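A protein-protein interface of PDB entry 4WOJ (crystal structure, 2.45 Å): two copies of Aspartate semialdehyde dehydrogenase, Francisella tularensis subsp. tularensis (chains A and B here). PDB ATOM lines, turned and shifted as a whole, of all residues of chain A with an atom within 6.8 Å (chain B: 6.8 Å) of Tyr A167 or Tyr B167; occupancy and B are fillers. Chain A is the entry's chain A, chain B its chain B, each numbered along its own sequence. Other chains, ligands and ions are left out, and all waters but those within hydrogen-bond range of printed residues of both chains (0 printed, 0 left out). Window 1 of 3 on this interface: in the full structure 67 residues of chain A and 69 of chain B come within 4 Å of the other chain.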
ATOM      1  N   SER A 164      -3.493 -20.076 -14.560  1.00  0.00           N
ATOM      2  CA  SER A 164      -4.545 -21.106 -14.598  1.00  0.00           C
ATOM      3  C   SER A 164      -4.208 -22.377 -13.788  1.00  0.00           C
ATOM      4  O   SER A 164      -3.131 -22.935 -13.938  1.00  0.00           O
ATOM      5  CB  SER A 164      -4.863 -21.520 -16.038  1.00  0.00           C
ATOM      6  OG  SER A 164      -5.679 -22.699 -16.061  1.00  0.00           O
ATOM      7  N   SER A 165      -5.164 -22.843 -12.983  1.00  0.00           N
ATOM      8  CA  SER A 165      -5.094 -24.134 -12.313  1.00  0.00           C
ATOM      9  C   SER A 165      -6.191 -25.012 -12.888  1.00  0.00           C
ATOM     10  O   SER A 165      -7.364 -24.708 -12.778  1.00  0.00           O
ATOM     11  CB  SER A 165      -5.278 -23.997 -10.788  1.00  0.00           C
ATOM     12  OG  SER A 165      -4.275 -23.182 -10.192  1.00  0.00           O
ATOM     13  N   THR A 166      -5.818 -26.074 -13.558  1.00  0.00           N
ATOM     14  CA  THR A 166      -6.813 -26.833 -14.296  1.00  0.00           C
ATOM     15  C   THR A 166      -7.216 -28.071 -13.521  1.00  0.00           C
ATOM     16  O   THR A 166      -6.501 -28.543 -12.622  1.00  0.00           O
ATOM     17  CB  THR A 166      -6.329 -27.267 -15.680  1.00  0.00           C
ATOM     18  OG1 THR A 166      -5.468 -28.396 -15.538  1.00  0.00           O
ATOM     19  CG2 THR A 166      -5.582 -26.116 -16.360  1.00  0.00           C
ATOM     20  N   TYR A 167      -8.402 -28.522 -13.877  1.00  0.00           N
ATOM     21  CA  TYR A 167      -9.066 -29.657 -13.302  1.00  0.00           C
ATOM     22  C   TYR A 167      -9.490 -30.383 -14.578  1.00  0.00           C
ATOM     23  O   TYR A 167     -10.595 -30.159 -15.103  1.00  0.00           O
ATOM     24  CB  TYR A 167     -10.316 -29.220 -12.528  1.00  0.00           C
ATOM     25  CG  TYR A 167     -10.135 -28.275 -11.331  1.00  0.00           C
ATOM     26  CD1 TYR A 167      -9.684 -26.965 -11.488  1.00  0.00           C
ATOM     27  CD2 TYR A 167     -10.452 -28.702 -10.052  1.00  0.00           C
ATOM     28  CE1 TYR A 167      -9.524 -26.119 -10.380  1.00  0.00           C
ATOM     29  CE2 TYR A 167     -10.292 -27.880  -8.950  1.00  0.00           C
ATOM     30  CZ  TYR A 167      -9.830 -26.583  -9.109  1.00  0.00           C
ATOM     31  OH  TYR A 167      -9.690 -25.785  -7.958  1.00  0.00           O
ATOM     32  N   GLN A 168      -8.561 -31.164 -15.132  1.00  0.00           N
ATOM     33  CA  GLN A 168      -8.728 -31.769 -16.456  1.00  0.00           C
ATOM     34  C   GLN A 168      -9.295 -33.155 -16.482  1.00  0.00           C
ATOM     35  O   GLN A 168      -8.892 -34.009 -15.738  1.00  0.00           O
ATOM     36  CB  GLN A 168      -7.400 -31.812 -17.140  1.00  0.00           C
ATOM     37  CG  GLN A 168      -6.959 -30.419 -17.518  1.00  0.00           C
ATOM     38  CD  GLN A 168      -5.616 -30.404 -18.163  1.00  0.00           C
ATOM     39  OE1 GLN A 168      -4.723 -29.672 -17.739  1.00  0.00           O
ATOM     40  NE2 GLN A 168      -5.463 -31.210 -19.216  1.00  0.00           N
ATOM     41  N   ALA A 169     -10.194 -33.365 -17.412  1.00  0.00           N
ATOM     42  CA  ALA A 169     -10.906 -34.620 -17.574  1.00  0.00           C
ATOM     43  C   ALA A 169     -10.105 -35.662 -18.371  1.00  0.00           C
ATOM     44  O   ALA A 169      -9.147 -35.372 -19.078  1.00  0.00           O
ATOM     45  CB  ALA A 169     -12.233 -34.378 -18.266  1.00  0.00           C
ATOM     46  N   LEU A 228      -6.436 -37.429  -7.603  1.00  0.00           N
ATOM     47  CA  LEU A 228      -6.012 -36.305  -8.416  1.00  0.00           C
ATOM     48  C   LEU A 228      -4.647 -36.643  -8.934  1.00  0.00           C
ATOM     49  O   LEU A 228      -3.855 -37.149  -8.175  1.00  0.00           O
ATOM     50  CB  LEU A 228      -5.834 -35.055  -7.502  1.00  0.00           C
ATOM     51  CG  LEU A 228      -6.940 -34.034  -7.414  1.00  0.00           C
ATOM     52  CD1 LEU A 228      -8.235 -34.720  -7.001  1.00  0.00           C
ATOM     53  CD2 LEU A 228      -6.602 -32.923  -6.431  1.00  0.00           C
ATOM     54  N   ILE A 266      -0.629 -24.780 -13.003  1.00  0.00           N
ATOM     55  CA  ILE A 266      -0.479 -26.185 -12.945  1.00  0.00           C
ATOM     56  C   ILE A 266      -1.649 -26.925 -13.580  1.00  0.00           C
ATOM     57  O   ILE A 266      -2.808 -26.519 -13.433  1.00  0.00           O
ATOM     58  CB  ILE A 266      -0.356 -26.640 -11.505  1.00  0.00           C
ATOM     59  CG1 ILE A 266       0.229 -28.050 -11.501  1.00  0.00           C
ATOM     60  CG2 ILE A 266      -1.717 -26.513 -10.830  1.00  0.00           C
ATOM     61  CD1 ILE A 266       0.148 -28.758 -10.173  1.00  0.00           C
ATOM     62  N   CYS A 267      -1.310 -27.989 -14.297  1.00  0.00           N
ATOM     63  CA  CYS A 267      -2.283 -28.829 -14.992  1.00  0.00           C
ATOM     64  C   CYS A 267      -2.495 -30.173 -14.216  1.00  0.00           C
ATOM     65  O   CYS A 267      -1.561 -30.890 -13.905  1.00  0.00           O
ATOM     66  CB  CYS A 267      -1.866 -29.040 -16.454  1.00  0.00           C
ATOM     67  SG  CYS A 267      -1.846 -27.529 -17.513  1.00  0.00           S
ATOM     68  N   VAL A 268      -3.732 -30.420 -13.827  1.00  0.00           N
ATOM     69  CA  VAL A 268      -4.050 -31.489 -12.917  1.00  0.00           C
ATOM     70  C   VAL A 268      -5.142 -32.320 -13.537  1.00  0.00           C
ATOM     71  O   VAL A 268      -6.159 -31.792 -13.994  1.00  0.00           O
ATOM     72  CB  VAL A 268      -4.549 -30.974 -11.548  1.00  0.00           C
ATOM     73  CG1 VAL A 268      -4.704 -32.115 -10.552  1.00  0.00           C
ATOM     74  CG2 VAL A 268      -3.609 -29.910 -10.976  1.00  0.00           C
ATOM     75  N   ARG A 269      -4.922 -33.625 -13.567  1.00  0.00           N
ATOM     76  CA  ARG A 269      -5.925 -34.541 -14.017  1.00  0.00           C
ATOM     77  C   ARG A 269      -6.818 -34.809 -12.846  1.00  0.00           C
ATOM     78  O   ARG A 269      -6.340 -35.050 -11.735  1.00  0.00           O
ATOM     79  CB  ARG A 269      -5.284 -35.850 -14.516  1.00  0.00           C
ATOM     80  CG  ARG A 269      -6.272 -36.816 -15.143  1.00  0.00           C
ATOM     81  CD  ARG A 269      -6.651 -36.402 -16.534  1.00  0.00           C
ATOM     82  NE  ARG A 269      -5.596 -36.732 -17.459  1.00  0.00           N
ATOM     83  CZ  ARG A 269      -5.408 -36.127 -18.623  1.00  0.00           C
ATOM     84  NH1 ARG A 269      -6.203 -35.134 -19.018  1.00  0.00           N
ATOM     85  NH2 ARG A 269      -4.392 -36.475 -19.384  1.00  0.00           N
ATOM     86  N   VAL A 270      -8.127 -34.779 -13.100  1.00  0.00           N
ATOM     87  CA  VAL A 270      -9.166 -35.123 -12.094  1.00  0.00           C
ATOM     88  C   VAL A 270     -10.144 -36.163 -12.671  1.00  0.00           C
ATOM     89  O   VAL A 270     -10.149 -36.405 -13.866  1.00  0.00           O
ATOM     90  CB  VAL A 270      -9.955 -33.870 -11.623  1.00  0.00           C
ATOM     91  CG1 VAL A 270      -9.031 -32.875 -10.950  1.00  0.00           C
ATOM     92  CG2 VAL A 270     -10.733 -33.248 -12.789  1.00  0.00           C
ATOM     93  N   SER A 272     -13.013 -36.438 -13.938  1.00  0.00           N
ATOM     94  CA  SER A 272     -14.096 -35.990 -14.791  1.00  0.00           C
ATOM     95  C   SER A 272     -13.954 -36.727 -16.105  1.00  0.00           C
ATOM     96  O   SER A 272     -12.884 -37.205 -16.436  1.00  0.00           O
ATOM     97  CB  SER A 272     -14.003 -34.475 -15.064  1.00  0.00           C
ATOM     98  OG  SER A 272     -14.321 -33.735 -13.901  1.00  0.00           O
ATOM     99  N   SER A 275     -15.203 -32.730 -19.714  1.00  0.00           N
ATOM    100  CA  SER A 275     -15.117 -31.271 -19.586  1.00  0.00           C
ATOM    101  C   SER A 275     -13.901 -30.861 -18.792  1.00  0.00           C
ATOM    102  O   SER A 275     -13.686 -31.378 -17.707  1.00  0.00           O
ATOM    103  CB  SER A 275     -16.393 -30.707 -18.964  1.00  0.00           C
ATOM    104  OG  SER A 275     -17.383 -30.462 -19.968  1.00  0.00           O
ATOM    105  N   HIS A 276     -13.109 -29.929 -19.336  1.00  0.00           N
ATOM    106  CA  HIS A 276     -12.031 -29.317 -18.565  1.00  0.00           C
ATOM    107  C   HIS A 276     -12.530 -28.118 -17.832  1.00  0.00           C
ATOM    108  O   HIS A 276     -13.265 -27.334 -18.396  1.00  0.00           O
ATOM    109  CB  HIS A 276     -10.887 -28.897 -19.444  1.00  0.00           C
ATOM    110  CG  HIS A 276     -10.159 -30.050 -20.041  1.00  0.00           C
ATOM    111  ND1 HIS A 276     -10.394 -31.351 -19.657  1.00  0.00           N
ATOM    112  CD2 HIS A 276      -9.189 -30.103 -20.978  1.00  0.00           C
ATOM    113  CE1 HIS A 276      -9.608 -32.164 -20.339  1.00  0.00           C
ATOM    114  NE2 HIS A 276      -8.856 -31.430 -21.140  1.00  0.00           N
ATOM    115  N   SER A 277     -12.145 -28.003 -16.568  1.00  0.00           N
ATOM    116  CA  SER A 277     -12.430 -26.825 -15.760  1.00  0.00           C
ATOM    117  C   SER A 277     -11.134 -26.100 -15.427  1.00  0.00           C
ATOM    118  O   SER A 277     -10.060 -26.688 -15.417  1.00  0.00           O
ATOM    119  CB  SER A 277     -13.186 -27.187 -14.485  1.00  0.00           C
ATOM    120  OG  SER A 277     -14.254 -28.086 -14.755  1.00  0.00           O
ATOM    121  N   GLN A 278     -11.254 -24.823 -15.114  1.00  0.00           N
ATOM    122  CA  GLN A 278     -10.118 -23.970 -14.895  1.00  0.00           C
ATOM    123  C   GLN A 278     -10.459 -22.812 -13.987  1.00  0.00           C
ATOM    124  O   GLN A 278     -11.357 -22.021 -14.312  1.00  0.00           O
ATOM    125  CB  GLN A 278      -9.663 -23.349 -16.223  1.00  0.00           C
ATOM    126  CG  GLN A 278      -8.851 -24.252 -17.093  1.00  0.00           C
ATOM    127  CD  GLN A 278      -8.355 -23.568 -18.325  1.00  0.00           C
ATOM    128  OE1 GLN A 278      -7.313 -22.955 -18.320  1.00  0.00           O
ATOM    129  NE2 GLN A 278      -9.087 -23.705 -19.399  1.00  0.00           N
ATOM    130  N   ALA A 279      -9.686 -22.687 -12.904  1.00  0.00           N
ATOM    131  CA  ALA A 279      -9.649 -21.493 -12.091  1.00  0.00           C
ATOM    132  C   ALA A 279      -8.612 -20.503 -12.647  1.00  0.00           C
ATOM    133  O   ALA A 279      -7.427 -20.795 -12.705  1.00  0.00           O
ATOM    134  CB  ALA A 279      -9.321 -21.842 -10.661  1.00  0.00           C
ATOM    135  N   PRO A 320     -18.842 -29.592 -14.966  1.00  0.00           N
ATOM    136  CA  PRO A 320     -18.723 -30.631 -16.001  1.00  0.00           C
ATOM    137  C   PRO A 320     -20.039 -31.325 -16.340  1.00  0.00           C
ATOM    138  O   PRO A 320     -20.353 -31.555 -17.523  1.00  0.00           O
ATOM    139  CB  PRO A 320     -17.763 -31.643 -15.379  1.00  0.00           C
ATOM    140  CG  PRO A 320     -16.957 -30.886 -14.396  1.00  0.00           C
ATOM    141  CD  PRO A 320     -17.789 -29.716 -13.944  1.00  0.00           C
ATOM    142  N   PHE A 347     -13.814 -18.745 -12.800  1.00  0.00           N
ATOM    143  CA  PHE A 347     -13.741 -20.223 -12.981  1.00  0.00           C
ATOM    144  C   PHE A 347     -14.525 -20.544 -14.248  1.00  0.00           C
ATOM    145  O   PHE A 347     -15.642 -20.096 -14.387  1.00  0.00           O
ATOM    146  CB  PHE A 347     -14.400 -20.976 -11.811  1.00  0.00           C
ATOM    147  CG  PHE A 347     -14.126 -22.478 -11.760  1.00  0.00           C
ATOM    148  CD1 PHE A 347     -12.959 -22.969 -11.209  1.00  0.00           C
ATOM    149  CD2 PHE A 347     -15.055 -23.398 -12.211  1.00  0.00           C
ATOM    150  CE1 PHE A 347     -12.727 -24.350 -11.127  1.00  0.00           C
ATOM    151  CE2 PHE A 347     -14.838 -24.787 -12.105  1.00  0.00           C
ATOM    152  CZ  PHE A 347     -13.674 -25.262 -11.543  1.00  0.00           C
ATOM    153  N   SER B 164      -4.481 -19.436  -4.022  1.00  0.00           N
ATOM    154  CA  SER B 164      -4.743 -20.865  -3.907  1.00  0.00           C
ATOM    155  C   SER B 164      -5.992 -21.295  -4.674  1.00  0.00           C
ATOM    156  O   SER B 164      -7.048 -20.690  -4.550  1.00  0.00           O
ATOM    157  CB  SER B 164      -4.886 -21.283  -2.457  1.00  0.00           C
ATOM    158  OG  SER B 164      -5.409 -22.624  -2.350  1.00  0.00           O
ATOM    159  N   SER B 165      -5.857 -22.340  -5.474  1.00  0.00           N
ATOM    160  CA  SER B 165      -6.995 -23.037  -6.102  1.00  0.00           C
ATOM    161  C   SER B 165      -7.076 -24.428  -5.462  1.00  0.00           C
ATOM    162  O   SER B 165      -6.156 -25.192  -5.559  1.00  0.00           O
ATOM    163  CB  SER B 165      -6.795 -23.191  -7.611  1.00  0.00           C
ATOM    164  OG  SER B 165      -6.642 -21.937  -8.274  1.00  0.00           O
ATOM    165  N   THR B 166      -8.178 -24.739  -4.797  1.00  0.00           N
ATOM    166  CA  THR B 166      -8.256 -25.925  -4.027  1.00  0.00           C
ATOM    167  C   THR B 166      -9.081 -26.980  -4.726  1.00  0.00           C
ATOM    168  O   THR B 166      -9.853 -26.698  -5.644  1.00  0.00           O
ATOM    169  CB  THR B 166      -8.862 -25.711  -2.649  1.00  0.00           C
ATOM    170  OG1 THR B 166     -10.282 -25.641  -2.766  1.00  0.00           O
ATOM    171  CG2 THR B 166      -8.312 -24.442  -2.004  1.00  0.00           C
ATOM    172  N   TYR B 167      -8.811 -28.197  -4.305  1.00  0.00           N
ATOM    173  CA  TYR B 167      -9.356 -29.411  -4.866  1.00  0.00           C
ATOM    174  C   TYR B 167      -9.681 -30.135  -3.598  1.00  0.00           C
ATOM    175  O   TYR B 167      -8.866 -30.864  -3.068  1.00  0.00           O
ATOM    176  CB  TYR B 167      -8.295 -30.175  -5.639  1.00  0.00           C
ATOM    177  CG  TYR B 167      -7.642 -29.499  -6.877  1.00  0.00           C
ATOM    178  CD1 TYR B 167      -6.790 -28.408  -6.770  1.00  0.00           C
ATOM    179  CD2 TYR B 167      -7.839 -30.033  -8.145  1.00  0.00           C
ATOM    180  CE1 TYR B 167      -6.197 -27.827  -7.910  1.00  0.00           C
ATOM    181  CE2 TYR B 167      -7.255 -29.480  -9.280  1.00  0.00           C
ATOM    182  CZ  TYR B 167      -6.433 -28.369  -9.159  1.00  0.00           C
ATOM    183  OH  TYR B 167      -5.904 -27.855 -10.327  1.00  0.00           O
ATOM    184  N   GLN B 168     -10.812 -29.779  -3.027  1.00  0.00           N
ATOM    185  CA  GLN B 168     -11.196 -30.194  -1.703  1.00  0.00           C
ATOM    186  C   GLN B 168     -12.065 -31.432  -1.597  1.00  0.00           C
ATOM    187  O   GLN B 168     -13.056 -31.587  -2.302  1.00  0.00           O
ATOM    188  CB  GLN B 168     -11.980 -29.085  -1.058  1.00  0.00           C
ATOM    189  CG  GLN B 168     -11.068 -27.949  -0.718  1.00  0.00           C
ATOM    190  CD  GLN B 168     -11.813 -26.818  -0.094  1.00  0.00           C
ATOM    191  OE1 GLN B 168     -11.692 -25.660  -0.543  1.00  0.00           O
ATOM    192  NE2 GLN B 168     -12.566 -27.119   0.978  1.00  0.00           N
ATOM    193  N   ALA B 169     -11.697 -32.276  -0.660  1.00  0.00           N
ATOM    194  CA  ALA B 169     -12.340 -33.576  -0.463  1.00  0.00           C
ATOM    195  C   ALA B 169     -13.631 -33.467   0.351  1.00  0.00           C
ATOM    196  O   ALA B 169     -13.902 -32.493   1.053  1.00  0.00           O
ATOM    197  CB  ALA B 169     -11.377 -34.509   0.219  1.00  0.00           C
ATOM    198  N   LEU B 228     -17.329 -31.768 -10.346  1.00  0.00           N
ATOM    199  CA  LEU B 228     -16.684 -30.881  -9.363  1.00  0.00           C
ATOM    200  C   LEU B 228     -17.599 -29.680  -9.069  1.00  0.00           C
ATOM    201  O   LEU B 228     -18.424 -29.332  -9.879  1.00  0.00           O
ATOM    202  CB  LEU B 228     -15.270 -30.477  -9.794  1.00  0.00           C
ATOM    203  CG  LEU B 228     -15.101 -29.762 -11.107  1.00  0.00           C
ATOM    204  CD1 LEU B 228     -15.542 -28.295 -11.025  1.00  0.00           C
ATOM    205  CD2 LEU B 228     -13.639 -29.832 -11.506  1.00  0.00           C
ATOM    206  N   ILE B 266      -9.935 -19.631  -5.531  1.00  0.00           N
ATOM    207  CA  ILE B 266     -11.187 -20.304  -5.508  1.00  0.00           C
ATOM    208  C   ILE B 266     -11.129 -21.655  -4.793  1.00  0.00           C
ATOM    209  O   ILE B 266     -10.170 -22.422  -4.951  1.00  0.00           O
ATOM    210  CB  ILE B 266     -11.667 -20.525  -6.921  1.00  0.00           C
ATOM    211  CG1 ILE B 266     -13.174 -20.843  -6.904  1.00  0.00           C
ATOM    212  CG2 ILE B 266     -10.835 -21.641  -7.571  1.00  0.00           C
ATOM    213  CD1 ILE B 266     -13.708 -21.352  -8.213  1.00  0.00           C
ATOM    214  N   CYS B 267     -12.208 -21.953  -4.072  1.00  0.00           N
ATOM    215  CA  CYS B 267     -12.371 -23.221  -3.388  1.00  0.00           C
ATOM    216  C   CYS B 267     -13.353 -24.165  -4.145  1.00  0.00           C
ATOM    217  O   CYS B 267     -14.489 -23.816  -4.407  1.00  0.00           O
ATOM    218  CB  CYS B 267     -12.769 -22.969  -1.921  1.00  0.00           C
ATOM    219  SG  CYS B 267     -11.492 -22.134  -0.912  1.00  0.00           S
ATOM    220  N   VAL B 268     -12.898 -25.367  -4.465  1.00  0.00           N
ATOM    221  CA  VAL B 268     -13.640 -26.285  -5.318  1.00  0.00           C
ATOM    222  C   VAL B 268     -13.734 -27.659  -4.666  1.00  0.00           C
ATOM    223  O   VAL B 268     -12.742 -28.200  -4.193  1.00  0.00           O
ATOM    224  CB  VAL B 268     -12.970 -26.465  -6.681  1.00  0.00           C
ATOM    225  CG1 VAL B 268     -13.864 -27.252  -7.650  1.00  0.00           C
ATOM    226  CG2 VAL B 268     -12.592 -25.100  -7.317  1.00  0.00           C
ATOM    227  N   ARG B 269     -14.943 -28.187  -4.619  1.00  0.00           N
ATOM    228  CA  ARG B 269     -15.165 -29.501  -4.139  1.00  0.00           C
ATOM    229  C   ARG B 269     -14.919 -30.475  -5.255  1.00  0.00           C
ATOM    230  O   ARG B 269     -15.377 -30.229  -6.400  1.00  0.00           O
ATOM    231  CB  ARG B 269     -16.612 -29.629  -3.656  1.00  0.00           C
ATOM    232  CG  ARG B 269     -16.836 -30.875  -2.883  1.00  0.00           C
ATOM    233  CD  ARG B 269     -16.137 -30.784  -1.560  1.00  0.00           C
ATOM    234  NE  ARG B 269     -16.937 -30.071  -0.586  1.00  0.00           N
ATOM    235  CZ  ARG B 269     -16.472 -29.635   0.575  1.00  0.00           C
ATOM    236  NH1 ARG B 269     -15.184 -29.770   0.905  1.00  0.00           N
ATOM    237  NH2 ARG B 269     -17.294 -29.024   1.409  1.00  0.00           N
ATOM    238  N   VAL B 270     -14.155 -31.534  -4.945  1.00  0.00           N
ATOM    239  CA  VAL B 270     -13.820 -32.608  -5.933  1.00  0.00           C
ATOM    240  C   VAL B 270     -14.088 -33.982  -5.326  1.00  0.00           C
ATOM    241  O   VAL B 270     -14.284 -34.061  -4.112  1.00  0.00           O
ATOM    242  CB  VAL B 270     -12.357 -32.564  -6.428  1.00  0.00           C
ATOM    243  CG1 VAL B 270     -12.058 -31.236  -7.131  1.00  0.00           C
ATOM    244  CG2 VAL B 270     -11.381 -32.830  -5.281  1.00  0.00           C
ATOM    245  N   SER B 272     -12.704 -36.447  -4.049  1.00  0.00           N
ATOM    246  CA  SER B 272     -11.733 -37.060  -3.177  1.00  0.00           C
ATOM    247  C   SER B 272     -12.400 -37.320  -1.841  1.00  0.00           C
ATOM    248  O   SER B 272     -13.397 -36.717  -1.510  1.00  0.00           O
ATOM    249  CB  SER B 272     -10.544 -36.118  -2.963  1.00  0.00           C
ATOM    250  OG  SER B 272      -9.775 -36.030  -4.127  1.00  0.00           O
ATOM    251  N   SER B 275      -8.276 -36.010   1.617  1.00  0.00           N
ATOM    252  CA  SER B 275      -7.148 -35.161   1.445  1.00  0.00           C
ATOM    253  C   SER B 275      -7.445 -33.910   0.599  1.00  0.00           C
ATOM    254  O   SER B 275      -8.037 -34.025  -0.470  1.00  0.00           O
ATOM    255  CB  SER B 275      -6.022 -35.956   0.841  1.00  0.00           C
ATOM    256  OG  SER B 275      -5.333 -36.616   1.873  1.00  0.00           O
ATOM    257  N   HIS B 276      -7.096 -32.725   1.125  1.00  0.00           N
ATOM    258  CA  HIS B 276      -7.257 -31.482   0.358  1.00  0.00           C
ATOM    259  C   HIS B 276      -6.018 -31.231  -0.415  1.00  0.00           C
ATOM    260  O   HIS B 276      -4.938 -31.359   0.134  1.00  0.00           O
ATOM    261  CB  HIS B 276      -7.550 -30.281   1.227  1.00  0.00           C
ATOM    262  CG  HIS B 276      -8.920 -30.309   1.835  1.00  0.00           C
ATOM    263  ND1 HIS B 276      -9.871 -31.235   1.481  1.00  0.00           N
ATOM    264  CD2 HIS B 276      -9.498 -29.523   2.771  1.00  0.00           C
ATOM    265  CE1 HIS B 276     -10.973 -31.023   2.172  1.00  0.00           C
ATOM    266  NE2 HIS B 276     -10.771 -29.993   2.967  1.00  0.00           N
ATOM    267  N   SER B 277      -6.188 -30.941  -1.697  1.00  0.00           N
ATOM    268  CA  SER B 277      -5.091 -30.559  -2.517  1.00  0.00           C
ATOM    269  C   SER B 277      -5.217 -29.073  -2.887  1.00  0.00           C
ATOM    270  O   SER B 277      -6.293 -28.484  -2.850  1.00  0.00           O
ATOM    271  CB  SER B 277      -4.980 -31.414  -3.761  1.00  0.00           C
ATOM    272  OG  SER B 277      -5.100 -32.777  -3.461  1.00  0.00           O
ATOM    273  N   GLN B 278      -4.093 -28.482  -3.228  1.00  0.00           N
ATOM    274  CA  GLN B 278      -4.005 -27.042  -3.463  1.00  0.00           C
ATOM    275  C   GLN B 278      -2.870 -26.745  -4.404  1.00  0.00           C
ATOM    276  O   GLN B 278      -1.738 -27.081  -4.109  1.00  0.00           O
ATOM    277  CB  GLN B 278      -3.712 -26.296  -2.144  1.00  0.00           C
ATOM    278  CG  GLN B 278      -4.914 -26.103  -1.257  1.00  0.00           C
ATOM    279  CD  GLN B 278      -4.671 -25.310  -0.007  1.00  0.00           C
ATOM    280  OE1 GLN B 278      -4.358 -25.849   1.028  1.00  0.00           O
ATOM    281  NE2 GLN B 278      -4.912 -24.011  -0.083  1.00  0.00           N
ATOM    282  N   ALA B 279      -3.194 -26.062  -5.495  1.00  0.00           N
ATOM    283  CA  ALA B 279      -2.242 -25.386  -6.345  1.00  0.00           C
ATOM    284  C   ALA B 279      -2.000 -23.937  -5.869  1.00  0.00           C
ATOM    285  O   ALA B 279      -2.892 -23.113  -5.825  1.00  0.00           O
ATOM    286  CB  ALA B 279      -2.736 -25.391  -7.771  1.00  0.00           C
ATOM    287  N   PRO B 320      -3.836 -37.503  -3.181  1.00  0.00           N
ATOM    288  CA  PRO B 320      -4.713 -37.875  -2.096  1.00  0.00           C
ATOM    289  C   PRO B 320      -4.567 -39.347  -1.717  1.00  0.00           C
ATOM    290  O   PRO B 320      -4.587 -39.701  -0.524  1.00  0.00           O
ATOM    291  CB  PRO B 320      -6.102 -37.630  -2.692  1.00  0.00           C
ATOM    292  CG  PRO B 320      -5.921 -36.547  -3.681  1.00  0.00           C
ATOM    293  CD  PRO B 320      -4.514 -36.625  -4.161  1.00  0.00           C
ATOM    294  N   PHE B 347       2.360 -27.278  -5.711  1.00  0.00           N
ATOM    295  CA  PHE B 347       1.117 -28.024  -5.468  1.00  0.00           C
ATOM    296  C   PHE B 347       1.302 -28.810  -4.187  1.00  0.00           C
ATOM    297  O   PHE B 347       2.295 -29.471  -4.037  1.00  0.00           O
ATOM    298  CB  PHE B 347       0.837 -29.016  -6.610  1.00  0.00           C
ATOM    299  CG  PHE B 347      -0.553 -29.593  -6.619  1.00  0.00           C
ATOM    300  CD1 PHE B 347      -1.602 -28.912  -7.175  1.00  0.00           C
ATOM    301  CD2 PHE B 347      -0.799 -30.896  -6.129  1.00  0.00           C
ATOM    302  CE1 PHE B 347      -2.873 -29.467  -7.203  1.00  0.00           C
ATOM    303  CE2 PHE B 347      -2.057 -31.455  -6.155  1.00  0.00           C
ATOM    304  CZ  PHE B 347      -3.107 -30.736  -6.692  1.00  0.00           C
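The backbone carbonyl oxygen (O) of Thr A166 sits at hydrogen-bond distance from the side-chain hydroxyl (OH) of Tyr B167.
OG of Ser A165 is in hydrogen-bond range of OG of Ser B165.
The side-chain hydroxyl (OH) of Tyr A167 sits at hydrogen-bond distance from the backbone carbonyl oxygen (O) of Thr B166 (2.5 Å).
The backbone carbonyl oxygen of Ser A277 is in hydrogen-bond range of the backbone NH of Tyr A167.
The side-chain hydroxyl (OG1) of Thr B166 lies within hydrogen-bond range of the backbone NH (N) of Val B268.
The backbone carbonyl oxygen of Ser B164 is in hydrogen-bond range of the backbone NH of Ile B266 (3.2 Å).
N of Ser B165 lies within hydrogen-bond range of O of Ala B279, 3.1 Å away.
N of Ser A165 is in hydrogen-bond range of O of Ala A279 (3.1 Å).
The backbone carbonyl oxygen (O) of Ile A266 lies within hydrogen-bond range of the backbone NH (N) of Thr A166.
C of Ser A165 touches OH of Tyr B167, at 3.8 Å.
Ser A165 touches Ala B279.
Tyr A167 touches Leu B228.
Val B268 touches Tyr A167 (CG2 to OH, 3.0 Å).
CD2 of Leu A228 touches CB of Tyr B167, at 3.3 Å.
CD2 of Leu A228 touches OG of Ser B277, 3.3 Å away.
OH of Tyr B167 touches CG2 of Val A268, at 3.1 Å.
CG2 of Val A268 touches CE1 of Phe B347, at 3.9 Å.
Phe A347 touches Leu B228 (CZ to CD1, 3.6 Å).
CD1 of Ile B266 touches CD1 of Phe A347, at 3.5 Å.
Of the printed residues of chain B, Tyr A167 touches Ser B165 (3.9 Å), Thr B166 (2.5 Å), Tyr B167 (3.4 Å), Leu B228 (3.5 Å) and Val B268 (3.0 Å).
Tyr B167 touches just these residues of chain A: Ser A165, Thr A166, Tyr A167, Leu A228 and Val A268.
Printed residues of chain A within 4 Å of Ser B277: Leu A228.
Of the printed residues of chain B, Phe A347 touches Leu B228 (3.6 Å), Ile B266 (3.5 Å) and Val B268 (3.9 Å).
Of the printed residues of chain A, Pro B320 touches Leu A228 (3.9 Å).
His B276 touches none of the printed residues of chain A.
The nearest residue of chain B that does not touch Tyr A167 is Val B270 (4.2 Å).
Of the 20 printed residues of chain A, 10 touch a printed residue of chain B.
Printed residues of chain A that touch a printed residue of chain B: Ser A165, Thr A166, Tyr A167, Leu A228, Ile A266, Val A268, Ser A277, Ala A279, Pro A320 and Phe A347.
Of the 20 printed residues of chain B, 11 touch a printed residue of chain A.
Hydrophobic or aromatic side chains of chain B within 4 Å of the printed part of chain A: Tyr B167, Leu B228, Ile B266, Val B268, Ala B279, Pro B320 and Phe B347.
Tyr A167 touches Val B268, and with the chains exchanged Val A268 touches Tyr B167.
Leu A228 touches Ser B272, but with the chains exchanged Ser A272 does not touch Leu B228 (4.6 Å).
Ile A266 touches Phe B347, and with the chains exchanged Phe A347 touches Ile B266.
Val A268 touches Phe B347, and with the chains exchanged Phe A347 touches Val B268.
Positions printed for both chains: 164, 165, 166, 167, 168, 169, 228, 266, 267, 268, 269, 270, 272, 275, 276, 277, 278, 279, 320 and 347.
Of the 24 pairs that touch across the chains among the printed residues, 22 have their exchanged pair printed and touching as well.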
